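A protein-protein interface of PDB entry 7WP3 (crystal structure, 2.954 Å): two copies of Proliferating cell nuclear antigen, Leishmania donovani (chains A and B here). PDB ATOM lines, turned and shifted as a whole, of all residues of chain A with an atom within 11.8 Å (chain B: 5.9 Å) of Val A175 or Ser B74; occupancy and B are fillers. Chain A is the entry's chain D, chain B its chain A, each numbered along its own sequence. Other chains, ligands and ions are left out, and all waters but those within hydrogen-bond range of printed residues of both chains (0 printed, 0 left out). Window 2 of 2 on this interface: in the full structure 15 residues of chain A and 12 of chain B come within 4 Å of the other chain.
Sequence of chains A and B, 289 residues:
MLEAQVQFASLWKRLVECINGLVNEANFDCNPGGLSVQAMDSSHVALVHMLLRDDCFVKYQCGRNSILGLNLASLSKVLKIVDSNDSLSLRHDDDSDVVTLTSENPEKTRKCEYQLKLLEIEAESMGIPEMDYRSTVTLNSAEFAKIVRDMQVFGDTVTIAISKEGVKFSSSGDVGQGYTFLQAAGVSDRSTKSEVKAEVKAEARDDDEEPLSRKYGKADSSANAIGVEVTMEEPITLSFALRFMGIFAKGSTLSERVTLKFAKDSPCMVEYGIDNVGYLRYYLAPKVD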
ATOM      1  N   ARG A 149      -7.537  -7.272 -23.986  1.00  0.00           N
ATOM      2  CA  ARG A 149      -6.588  -6.388 -24.724  1.00  0.00           C
ATOM      3  C   ARG A 149      -7.005  -4.924 -24.509  1.00  0.00           C
ATOM      4  O   ARG A 149      -6.147  -4.115 -24.108  1.00  0.00           O
ATOM      5  CB  ARG A 149      -6.545  -6.749 -26.213  1.00  0.00           C
ATOM      6  CG  ARG A 149      -5.623  -5.864 -27.044  1.00  0.00           C
ATOM      7  CD  ARG A 149      -6.030  -5.768 -28.508  1.00  0.00           C
ATOM      8  NE  ARG A 149      -7.272  -5.018 -28.679  1.00  0.00           N
ATOM      9  CZ  ARG A 149      -7.895  -4.813 -29.839  1.00  0.00           C
ATOM     10  NH1 ARG A 149      -7.400  -5.309 -30.960  1.00  0.00           N
ATOM     11  NH2 ARG A 149      -9.019  -4.115 -29.870  1.00  0.00           N
ATOM     12  N   ASP A 150      -8.272  -4.598 -24.766  1.00  0.00           N
ATOM     13  CA  ASP A 150      -8.845  -3.239 -24.566  1.00  0.00           C
ATOM     14  C   ASP A 150      -8.594  -2.770 -23.133  1.00  0.00           C
ATOM     15  O   ASP A 150      -7.955  -1.720 -22.977  1.00  0.00           O
ATOM     16  CB  ASP A 150     -10.350  -3.192 -24.842  1.00  0.00           C
ATOM     17  CG  ASP A 150     -10.746  -3.485 -26.283  1.00  0.00           C
ATOM     18  OD1 ASP A 150      -9.844  -3.906 -27.066  1.00  0.00           O
ATOM     19  OD2 ASP A 150     -11.956  -3.280 -26.616  1.00  0.00           O
ATOM     20  N   MET A 151      -9.084  -3.503 -22.126  1.00  0.00           N
ATOM     21  CA  MET A 151      -8.976  -3.073 -20.700  1.00  0.00           C
ATOM     22  C   MET A 151      -7.501  -2.803 -20.380  1.00  0.00           C
ATOM     23  O   MET A 151      -7.238  -1.866 -19.625  1.00  0.00           O
ATOM     24  CB  MET A 151      -9.527  -4.102 -19.705  1.00  0.00           C
ATOM     25  CG  MET A 151     -11.005  -4.409 -19.873  1.00  0.00           C
ATOM     26  SD  MET A 151     -12.062  -2.986 -20.289  1.00  0.00           S
ATOM     27  CE  MET A 151     -11.842  -1.933 -18.863  1.00  0.00           C
ATOM     28  N   GLN A 152      -6.583  -3.560 -20.982  1.00  0.00           N
ATOM     29  CA  GLN A 152      -5.119  -3.423 -20.756  1.00  0.00           C
ATOM     30  C   GLN A 152      -4.587  -2.082 -21.269  1.00  0.00           C
ATOM     31  O   GLN A 152      -3.475  -1.704 -20.835  1.00  0.00           O
ATOM     32  CB  GLN A 152      -4.336  -4.538 -21.443  1.00  0.00           C
ATOM     33  CG  GLN A 152      -4.255  -5.787 -20.599  1.00  0.00           C
ATOM     34  CD  GLN A 152      -3.596  -6.927 -21.330  1.00  0.00           C
ATOM     35  OE1 GLN A 152      -4.040  -7.342 -22.408  1.00  0.00           O
ATOM     36  NE2 GLN A 152      -2.552  -7.464 -20.709  1.00  0.00           N
ATOM     37  N   VAL A 153      -5.295  -1.385 -22.163  1.00  0.00           N
ATOM     38  CA  VAL A 153      -4.815  -0.044 -22.616  1.00  0.00           C
ATOM     39  C   VAL A 153      -4.902   0.912 -21.426  1.00  0.00           C
ATOM     40  O   VAL A 153      -4.273   1.978 -21.510  1.00  0.00           O
ATOM     41  CB  VAL A 153      -5.548   0.530 -23.843  1.00  0.00           C
ATOM     42  CG1 VAL A 153      -5.787  -0.531 -24.906  1.00  0.00           C
ATOM     43  CG2 VAL A 153      -6.835   1.243 -23.472  1.00  0.00           C
ATOM     44  N   PHE A 154      -5.642   0.530 -20.374  1.00  0.00           N
ATOM     45  CA  PHE A 154      -5.903   1.363 -19.165  1.00  0.00           C
ATOM     46  C   PHE A 154      -5.004   0.940 -17.996  1.00  0.00           C
ATOM     47  O   PHE A 154      -4.291   1.807 -17.462  1.00  0.00           O
ATOM     48  CB  PHE A 154      -7.389   1.330 -18.798  1.00  0.00           C
ATOM     49  CG  PHE A 154      -8.253   1.912 -19.879  1.00  0.00           C
ATOM     50  CD1 PHE A 154      -8.313   3.285 -20.051  1.00  0.00           C
ATOM     51  CD2 PHE A 154      -8.932   1.094 -20.767  1.00  0.00           C
ATOM     52  CE1 PHE A 154      -9.070   3.835 -21.072  1.00  0.00           C
ATOM     53  CE2 PHE A 154      -9.691   1.643 -21.788  1.00  0.00           C
ATOM     54  CZ  PHE A 154      -9.760   3.013 -21.936  1.00  0.00           C
ATOM     55  N   GLY A 155      -5.016  -0.340 -17.626  1.00  0.00           N
ATOM     56  CA  GLY A 155      -4.347  -0.829 -16.409  1.00  0.00           C
ATOM     57  C   GLY A 155      -3.803  -2.235 -16.567  1.00  0.00           C
ATOM     58  O   GLY A 155      -3.572  -2.685 -17.707  1.00  0.00           O
ATOM     59  N   ASP A 156      -3.565  -2.891 -15.434  1.00  0.00           N
ATOM     60  CA  ASP A 156      -2.963  -4.247 -15.348  1.00  0.00           C
ATOM     61  C   ASP A 156      -3.929  -5.173 -14.606  1.00  0.00           C
ATOM     62  O   ASP A 156      -3.634  -6.383 -14.556  1.00  0.00           O
ATOM     63  CB  ASP A 156      -1.621  -4.184 -14.625  1.00  0.00           C
ATOM     64  CG  ASP A 156      -1.754  -3.588 -13.233  1.00  0.00           C
ATOM     65  OD1 ASP A 156      -2.906  -3.287 -12.826  1.00  0.00           O
ATOM     66  OD2 ASP A 156      -0.716  -3.425 -12.566  1.00  0.00           O
ATOM     67  N   SER A 171     -11.521  -1.178 -15.936  1.00  0.00           N
ATOM     68  CA  SER A 171     -10.070  -0.985 -15.649  1.00  0.00           C
ATOM     69  C   SER A 171      -9.745   0.505 -15.599  1.00  0.00           C
ATOM     70  O   SER A 171     -10.531   1.274 -16.160  1.00  0.00           O
ATOM     71  CB  SER A 171      -9.204  -1.674 -16.658  1.00  0.00           C
ATOM     72  OG  SER A 171      -7.837  -1.427 -16.365  1.00  0.00           O
ATOM     73  N   SER A 172      -8.644   0.885 -14.940  1.00  0.00           N
ATOM     74  CA  SER A 172      -8.245   2.306 -14.727  1.00  0.00           C
ATOM     75  C   SER A 172      -6.726   2.455 -14.666  1.00  0.00           C
ATOM     76  O   SER A 172      -6.070   1.572 -14.106  1.00  0.00           O
ATOM     77  CB  SER A 172      -8.862   2.854 -13.485  1.00  0.00           C
ATOM     78  OG  SER A 172     -10.266   2.878 -13.615  1.00  0.00           O
ATOM     79  N   GLY A 173      -6.208   3.562 -15.200  1.00  0.00           N
ATOM     80  CA  GLY A 173      -4.763   3.866 -15.260  1.00  0.00           C
ATOM     81  C   GLY A 173      -4.520   5.281 -15.759  1.00  0.00           C
ATOM     82  O   GLY A 173      -5.492   6.081 -15.777  1.00  0.00           O
ATOM     83  N   ASP A 174      -3.289   5.596 -16.164  1.00  0.00           N
ATOM     84  CA  ASP A 174      -2.914   6.985 -16.549  1.00  0.00           C
ATOM     85  C   ASP A 174      -3.785   7.420 -17.726  1.00  0.00           C
ATOM     86  O   ASP A 174      -4.420   8.498 -17.651  1.00  0.00           O
ATOM     87  CB  ASP A 174      -1.424   7.107 -16.878  1.00  0.00           C
ATOM     88  CG  ASP A 174      -0.548   7.011 -15.641  1.00  0.00           C
ATOM     89  OD1 ASP A 174      -1.037   6.451 -14.638  1.00  0.00           O
ATOM     90  OD2 ASP A 174       0.607   7.506 -15.682  1.00  0.00           O
ATOM     91  N   VAL A 175      -3.858   6.572 -18.750  1.00  0.00           N
ATOM     92  CA  VAL A 175      -4.662   6.846 -19.973  1.00  0.00           C
ATOM     93  C   VAL A 175      -6.040   7.322 -19.514  1.00  0.00           C
ATOM     94  O   VAL A 175      -6.606   8.228 -20.147  1.00  0.00           O
ATOM     95  CB  VAL A 175      -4.755   5.607 -20.876  1.00  0.00           C
ATOM     96  CG1 VAL A 175      -5.652   5.873 -22.073  1.00  0.00           C
ATOM     97  CG2 VAL A 175      -3.385   5.129 -21.337  1.00  0.00           C
ATOM     98  N   GLY A 176      -6.532   6.745 -18.423  1.00  0.00           N
ATOM     99  CA  GLY A 176      -7.823   7.102 -17.815  1.00  0.00           C
ATOM    100  C   GLY A 176      -8.559   5.865 -17.368  1.00  0.00           C
ATOM    101  O   GLY A 176      -7.902   4.895 -16.940  1.00  0.00           O
ATOM    102  N   GLN A 177      -9.881   5.897 -17.468  1.00  0.00           N
ATOM    103  CA  GLN A 177     -10.747   4.794 -16.992  1.00  0.00           C
ATOM    104  C   GLN A 177     -11.682   4.436 -18.136  1.00  0.00           C
ATOM    105  O   GLN A 177     -12.103   5.338 -18.862  1.00  0.00           O
ATOM    106  CB  GLN A 177     -11.488   5.190 -15.717  1.00  0.00           C
ATOM    107  CG  GLN A 177     -12.053   6.597 -15.764  1.00  0.00           C
ATOM    108  CD  GLN A 177     -12.513   7.052 -14.406  1.00  0.00           C
ATOM    109  OE1 GLN A 177     -12.437   6.311 -13.429  1.00  0.00           O
ATOM    110  NE2 GLN A 177     -13.008   8.280 -14.343  1.00  0.00           N
ATOM    111  N   GLY A 178     -11.949   3.149 -18.293  1.00  0.00           N
ATOM    112  CA  GLY A 178     -12.904   2.629 -19.280  1.00  0.00           C
ATOM    113  C   GLY A 178     -13.639   1.418 -18.748  1.00  0.00           C
ATOM    114  O   GLY A 178     -13.234   0.873 -17.699  1.00  0.00           O
ATOM    115  N   TYR A 179     -14.681   1.002 -19.458  1.00  0.00           N
ATOM    116  CA  TYR A 179     -15.409  -0.253 -19.170  1.00  0.00           C
ATOM    117  C   TYR A 179     -16.114  -0.752 -20.422  1.00  0.00           C
ATOM    118  O   TYR A 179     -16.418   0.038 -21.316  1.00  0.00           O
ATOM    119  CB  TYR A 179     -16.394  -0.049 -18.019  1.00  0.00           C
ATOM    120  CG  TYR A 179     -17.703   0.615 -18.353  1.00  0.00           C
ATOM    121  CD1 TYR A 179     -18.713  -0.080 -18.995  1.00  0.00           C
ATOM    122  CD2 TYR A 179     -17.958   1.918 -17.951  1.00  0.00           C
ATOM    123  CE1 TYR A 179     -19.928   0.524 -19.276  1.00  0.00           C
ATOM    124  CE2 TYR A 179     -19.177   2.527 -18.198  1.00  0.00           C
ATOM    125  CZ  TYR A 179     -20.165   1.829 -18.870  1.00  0.00           C
ATOM    126  OH  TYR A 179     -21.369   2.433 -19.125  1.00  0.00           O
ATOM    127  N   LEU A 242      -4.796  -8.798 -15.553  1.00  0.00           N
ATOM    128  CA  LEU A 242      -5.054  -8.789 -17.018  1.00  0.00           C
ATOM    129  C   LEU A 242      -3.933  -9.525 -17.748  1.00  0.00           C
ATOM    130  O   LEU A 242      -4.197 -10.131 -18.803  1.00  0.00           O
ATOM    131  CB  LEU A 242      -5.174  -7.354 -17.521  1.00  0.00           C
ATOM    132  CG  LEU A 242      -6.554  -6.741 -17.330  1.00  0.00           C
ATOM    133  CD1 LEU A 242      -6.489  -5.229 -17.445  1.00  0.00           C
ATOM    134  CD2 LEU A 242      -7.527  -7.310 -18.340  1.00  0.00           C
ATOM    135  N   ASN B  24       0.494  16.682 -29.549  1.00  0.00           N
ATOM    136  CA  ASN B  24       0.159  15.586 -28.585  1.00  0.00           C
ATOM    137  C   ASN B  24      -1.053  15.950 -27.739  1.00  0.00           C
ATOM    138  O   ASN B  24      -1.728  15.041 -27.206  1.00  0.00           O
ATOM    139  CB  ASN B  24       1.334  15.243 -27.680  1.00  0.00           C
ATOM    140  CG  ASN B  24       2.464  14.724 -28.532  1.00  0.00           C
ATOM    141  OD1 ASN B  24       2.221  14.123 -29.590  1.00  0.00           O
ATOM    142  ND2 ASN B  24       3.686  15.009 -28.111  1.00  0.00           N
ATOM    143  N   ASN B  71      -5.497  15.217 -24.344  1.00  0.00           N
ATOM    144  CA  ASN B  71      -4.250  14.481 -24.662  1.00  0.00           C
ATOM    145  C   ASN B  71      -4.531  13.551 -25.841  1.00  0.00           C
ATOM    146  O   ASN B  71      -5.063  12.453 -25.637  1.00  0.00           O
ATOM    147  CB  ASN B  71      -3.693  13.709 -23.473  1.00  0.00           C
ATOM    148  CG  ASN B  71      -2.307  13.189 -23.760  1.00  0.00           C
ATOM    149  OD1 ASN B  71      -1.533  13.824 -24.477  1.00  0.00           O
ATOM    150  ND2 ASN B  71      -1.981  12.046 -23.191  1.00  0.00           N
ATOM    151  N   LEU B  72      -4.181  14.003 -27.040  1.00  0.00           N
ATOM    152  CA  LEU B  72      -4.387  13.253 -28.298  1.00  0.00           C
ATOM    153  C   LEU B  72      -3.662  11.917 -28.193  1.00  0.00           C
ATOM    154  O   LEU B  72      -4.124  10.955 -28.813  1.00  0.00           O
ATOM    155  CB  LEU B  72      -3.874  14.090 -29.467  1.00  0.00           C
ATOM    156  CG  LEU B  72      -4.633  15.401 -29.673  1.00  0.00           C
ATOM    157  CD1 LEU B  72      -4.057  16.178 -30.841  1.00  0.00           C
ATOM    158  CD2 LEU B  72      -6.113  15.145 -29.894  1.00  0.00           C
ATOM    159  N   ALA B  73      -2.604  11.845 -27.390  1.00  0.00           N
ATOM    160  CA  ALA B  73      -1.900  10.573 -27.128  1.00  0.00           C
ATOM    161  C   ALA B  73      -2.911   9.567 -26.586  1.00  0.00           C
ATOM    162  O   ALA B  73      -3.155   8.556 -27.271  1.00  0.00           O
ATOM    163  CB  ALA B  73      -0.783  10.795 -26.162  1.00  0.00           C
ATOM    164  N   SER B  74      -3.503   9.878 -25.429  1.00  0.00           N
ATOM    165  CA  SER B  74      -4.473   9.004 -24.714  1.00  0.00           C
ATOM    166  C   SER B  74      -5.683   8.766 -25.604  1.00  0.00           C
ATOM    167  O   SER B  74      -6.106   7.605 -25.757  1.00  0.00           O
ATOM    168  CB  SER B  74      -4.914   9.619 -23.442  1.00  0.00           C
ATOM    169  OG  SER B  74      -3.790  10.128 -22.758  1.00  0.00           O
ATOM    170  N   LEU B  75      -6.220   9.847 -26.160  1.00  0.00           N
ATOM    171  CA  LEU B  75      -7.398   9.752 -27.046  1.00  0.00           C
ATOM    172  C   LEU B  75      -7.090   8.726 -28.142  1.00  0.00           C
ATOM    173  O   LEU B  75      -7.904   7.802 -28.328  1.00  0.00           O
ATOM    174  CB  LEU B  75      -7.719  11.135 -27.606  1.00  0.00           C
ATOM    175  CG  LEU B  75      -8.926  11.203 -28.539  1.00  0.00           C
ATOM    176  CD1 LEU B  75     -10.173  10.669 -27.866  1.00  0.00           C
ATOM    177  CD2 LEU B  75      -9.159  12.630 -29.010  1.00  0.00           C
ATOM    178  N   SER B  76      -5.934   8.841 -28.801  1.00  0.00           N
ATOM    179  CA  SER B  76      -5.464   7.837 -29.796  1.00  0.00           C
ATOM    180  C   SER B  76      -5.527   6.433 -29.178  1.00  0.00           C
ATOM    181  O   SER B  76      -6.226   5.556 -29.734  1.00  0.00           O
ATOM    182  CB  SER B  76      -4.087   8.140 -30.302  1.00  0.00           C
ATOM    183  OG  SER B  76      -3.815   7.388 -31.476  1.00  0.00           O
ATOM    184  N   LYS B  77      -4.876   6.248 -28.031  1.00  0.00           N
ATOM    185  CA  LYS B  77      -4.738   4.927 -27.366  1.00  0.00           C
ATOM    186  C   LYS B  77      -6.118   4.307 -27.122  1.00  0.00           C
ATOM    187  O   LYS B  77      -6.189   3.073 -27.026  1.00  0.00           O
ATOM    188  CB  LYS B  77      -3.970   5.074 -26.053  1.00  0.00           C
ATOM    189  CG  LYS B  77      -2.462   5.244 -26.178  1.00  0.00           C
ATOM    190  CD  LYS B  77      -1.772   5.119 -24.826  1.00  0.00           C
ATOM    191  CE  LYS B  77      -0.266   5.230 -24.885  1.00  0.00           C
ATOM    192  NZ  LYS B  77       0.174   6.644 -24.885  1.00  0.00           N
ATOM    193  N   VAL B  78      -7.161   5.125 -27.000  1.00  0.00           N
ATOM    194  CA  VAL B  78      -8.545   4.659 -26.699  1.00  0.00           C
ATOM    195  C   VAL B  78      -9.234   4.313 -28.013  1.00  0.00           C
ATOM    196  O   VAL B  78      -9.886   3.268 -28.105  1.00  0.00           O
ATOM    197  CB  VAL B  78      -9.386   5.717 -25.955  1.00  0.00           C
ATOM    198  CG1 VAL B  78     -10.831   5.264 -25.810  1.00  0.00           C
ATOM    199  CG2 VAL B  78      -8.820   6.082 -24.592  1.00  0.00           C
ATOM    200  N   LEU B  79      -9.187   5.224 -28.967  1.00  0.00           N
ATOM    201  CA  LEU B  79      -9.930   5.028 -30.227  1.00  0.00           C
ATOM    202  C   LEU B  79      -9.373   3.794 -30.939  1.00  0.00           C
ATOM    203  O   LEU B  79     -10.163   3.150 -31.654  1.00  0.00           O
ATOM    204  CB  LEU B  79      -9.818   6.298 -31.068  1.00  0.00           C
ATOM    205  CG  LEU B  79     -10.474   7.505 -30.424  1.00  0.00           C
ATOM    206  CD1 LEU B  79     -10.295   8.736 -31.273  1.00  0.00           C
ATOM    207  CD2 LEU B  79     -11.939   7.230 -30.200  1.00  0.00           C
ATOM    208  N   GLN B 115     -13.453   7.454 -19.946  1.00  0.00           N
ATOM    209  CA  GLN B 115     -13.347   8.847 -19.461  1.00  0.00           C
ATOM    210  C   GLN B 115     -11.894   9.286 -19.557  1.00  0.00           C
ATOM    211  O   GLN B 115     -11.016   8.560 -19.027  1.00  0.00           O
ATOM    212  CB  GLN B 115     -13.803   8.959 -18.011  1.00  0.00           C
ATOM    213  CG  GLN B 115     -15.201   8.421 -17.796  1.00  0.00           C
ATOM    214  CD  GLN B 115     -15.717   8.759 -16.427  1.00  0.00           C
ATOM    215  OE1 GLN B 115     -15.025   9.370 -15.613  1.00  0.00           O
ATOM    216  NE2 GLN B 115     -16.948   8.344 -16.175  1.00  0.00           N
ATOM    217  N   LEU B 116     -11.661  10.440 -20.175  1.00  0.00           N
ATOM    218  CA  LEU B 116     -10.309  11.035 -20.295  1.00  0.00           C
ATOM    219  C   LEU B 116     -10.265  12.343 -19.507  1.00  0.00           C
ATOM    220  O   LEU B 116     -11.158  13.186 -19.727  1.00  0.00           O
ATOM    221  CB  LEU B 116     -10.015  11.258 -21.776  1.00  0.00           C
ATOM    222  CG  LEU B 116     -10.171  10.009 -22.630  1.00  0.00           C
ATOM    223  CD1 LEU B 116     -10.070  10.351 -24.105  1.00  0.00           C
ATOM    224  CD2 LEU B 116      -9.131   8.973 -22.222  1.00  0.00           C
ATOM    225  N   LYS B 117      -9.258  12.503 -18.644  1.00  0.00           N
ATOM    226  CA  LYS B 117      -8.994  13.777 -17.931  1.00  0.00           C
ATOM    227  C   LYS B 117      -8.733  14.886 -18.951  1.00  0.00           C
ATOM    228  O   LYS B 117      -7.997  14.642 -19.912  1.00  0.00           O
ATOM    229  CB  LYS B 117      -7.801  13.645 -16.979  1.00  0.00           C
ATOM    230  CG  LYS B 117      -8.126  13.059 -15.608  1.00  0.00           C
ATOM    231  CD  LYS B 117      -9.099  13.913 -14.789  1.00  0.00           C
ATOM    232  CE  LYS B 117      -9.356  13.426 -13.376  1.00  0.00           C
ATOM    233  NZ  LYS B 117      -9.903  12.050 -13.340  1.00  0.00           N
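The side-chain amide nitrogen (ND2) of Asn B71 lies within hydrogen-bond range of the side-chain hydroxyl (OG) of Ser B74, at 2.7 Å.
Ser B74 touches Val A175.
Val A175 touches Lys B77 (CG2 to CD, 3.8 Å).
Val A175 touches Leu B116 (O to CD2, 3.4 Å).
O of Gln B115 touches CA of Gly A176 (3.7 Å).
Hydrophobic or aromatic side chains of chain A within 4 Å of the printed part of chain B: Val A175.
Hydrophobic or aromatic side chains of chain B within 4 Å of the printed part of chain A: Leu B116.
Among the printed residues, no Asp or Glu carboxylate lies within 4 Å of a Lys or Arg side-chain nitrogen of the other chain.
Of the printed residues of chain B, Gly A176 touches Gln B115.
Of the printed residues of chain B, Gln A177 touches Gln B115 (2.6 Å).
No residue of chain A comes within 4 Å of Asn B71.
Of chain A, only Val A175 comes within 4 Å of Ser B74.
Lys B77 touches just one residue of chain A: Val A175.
No residue of chain A comes within 4 Å of Val B78.
No position is printed for both chains.
Of the 5 pairs that touch across the chains among the printed residues, none has its exchanged pair printed and touching as well.
NE2 of Gln A177 is in hydrogen-bond range of OE1 of Gln B115 (2.6 Å).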
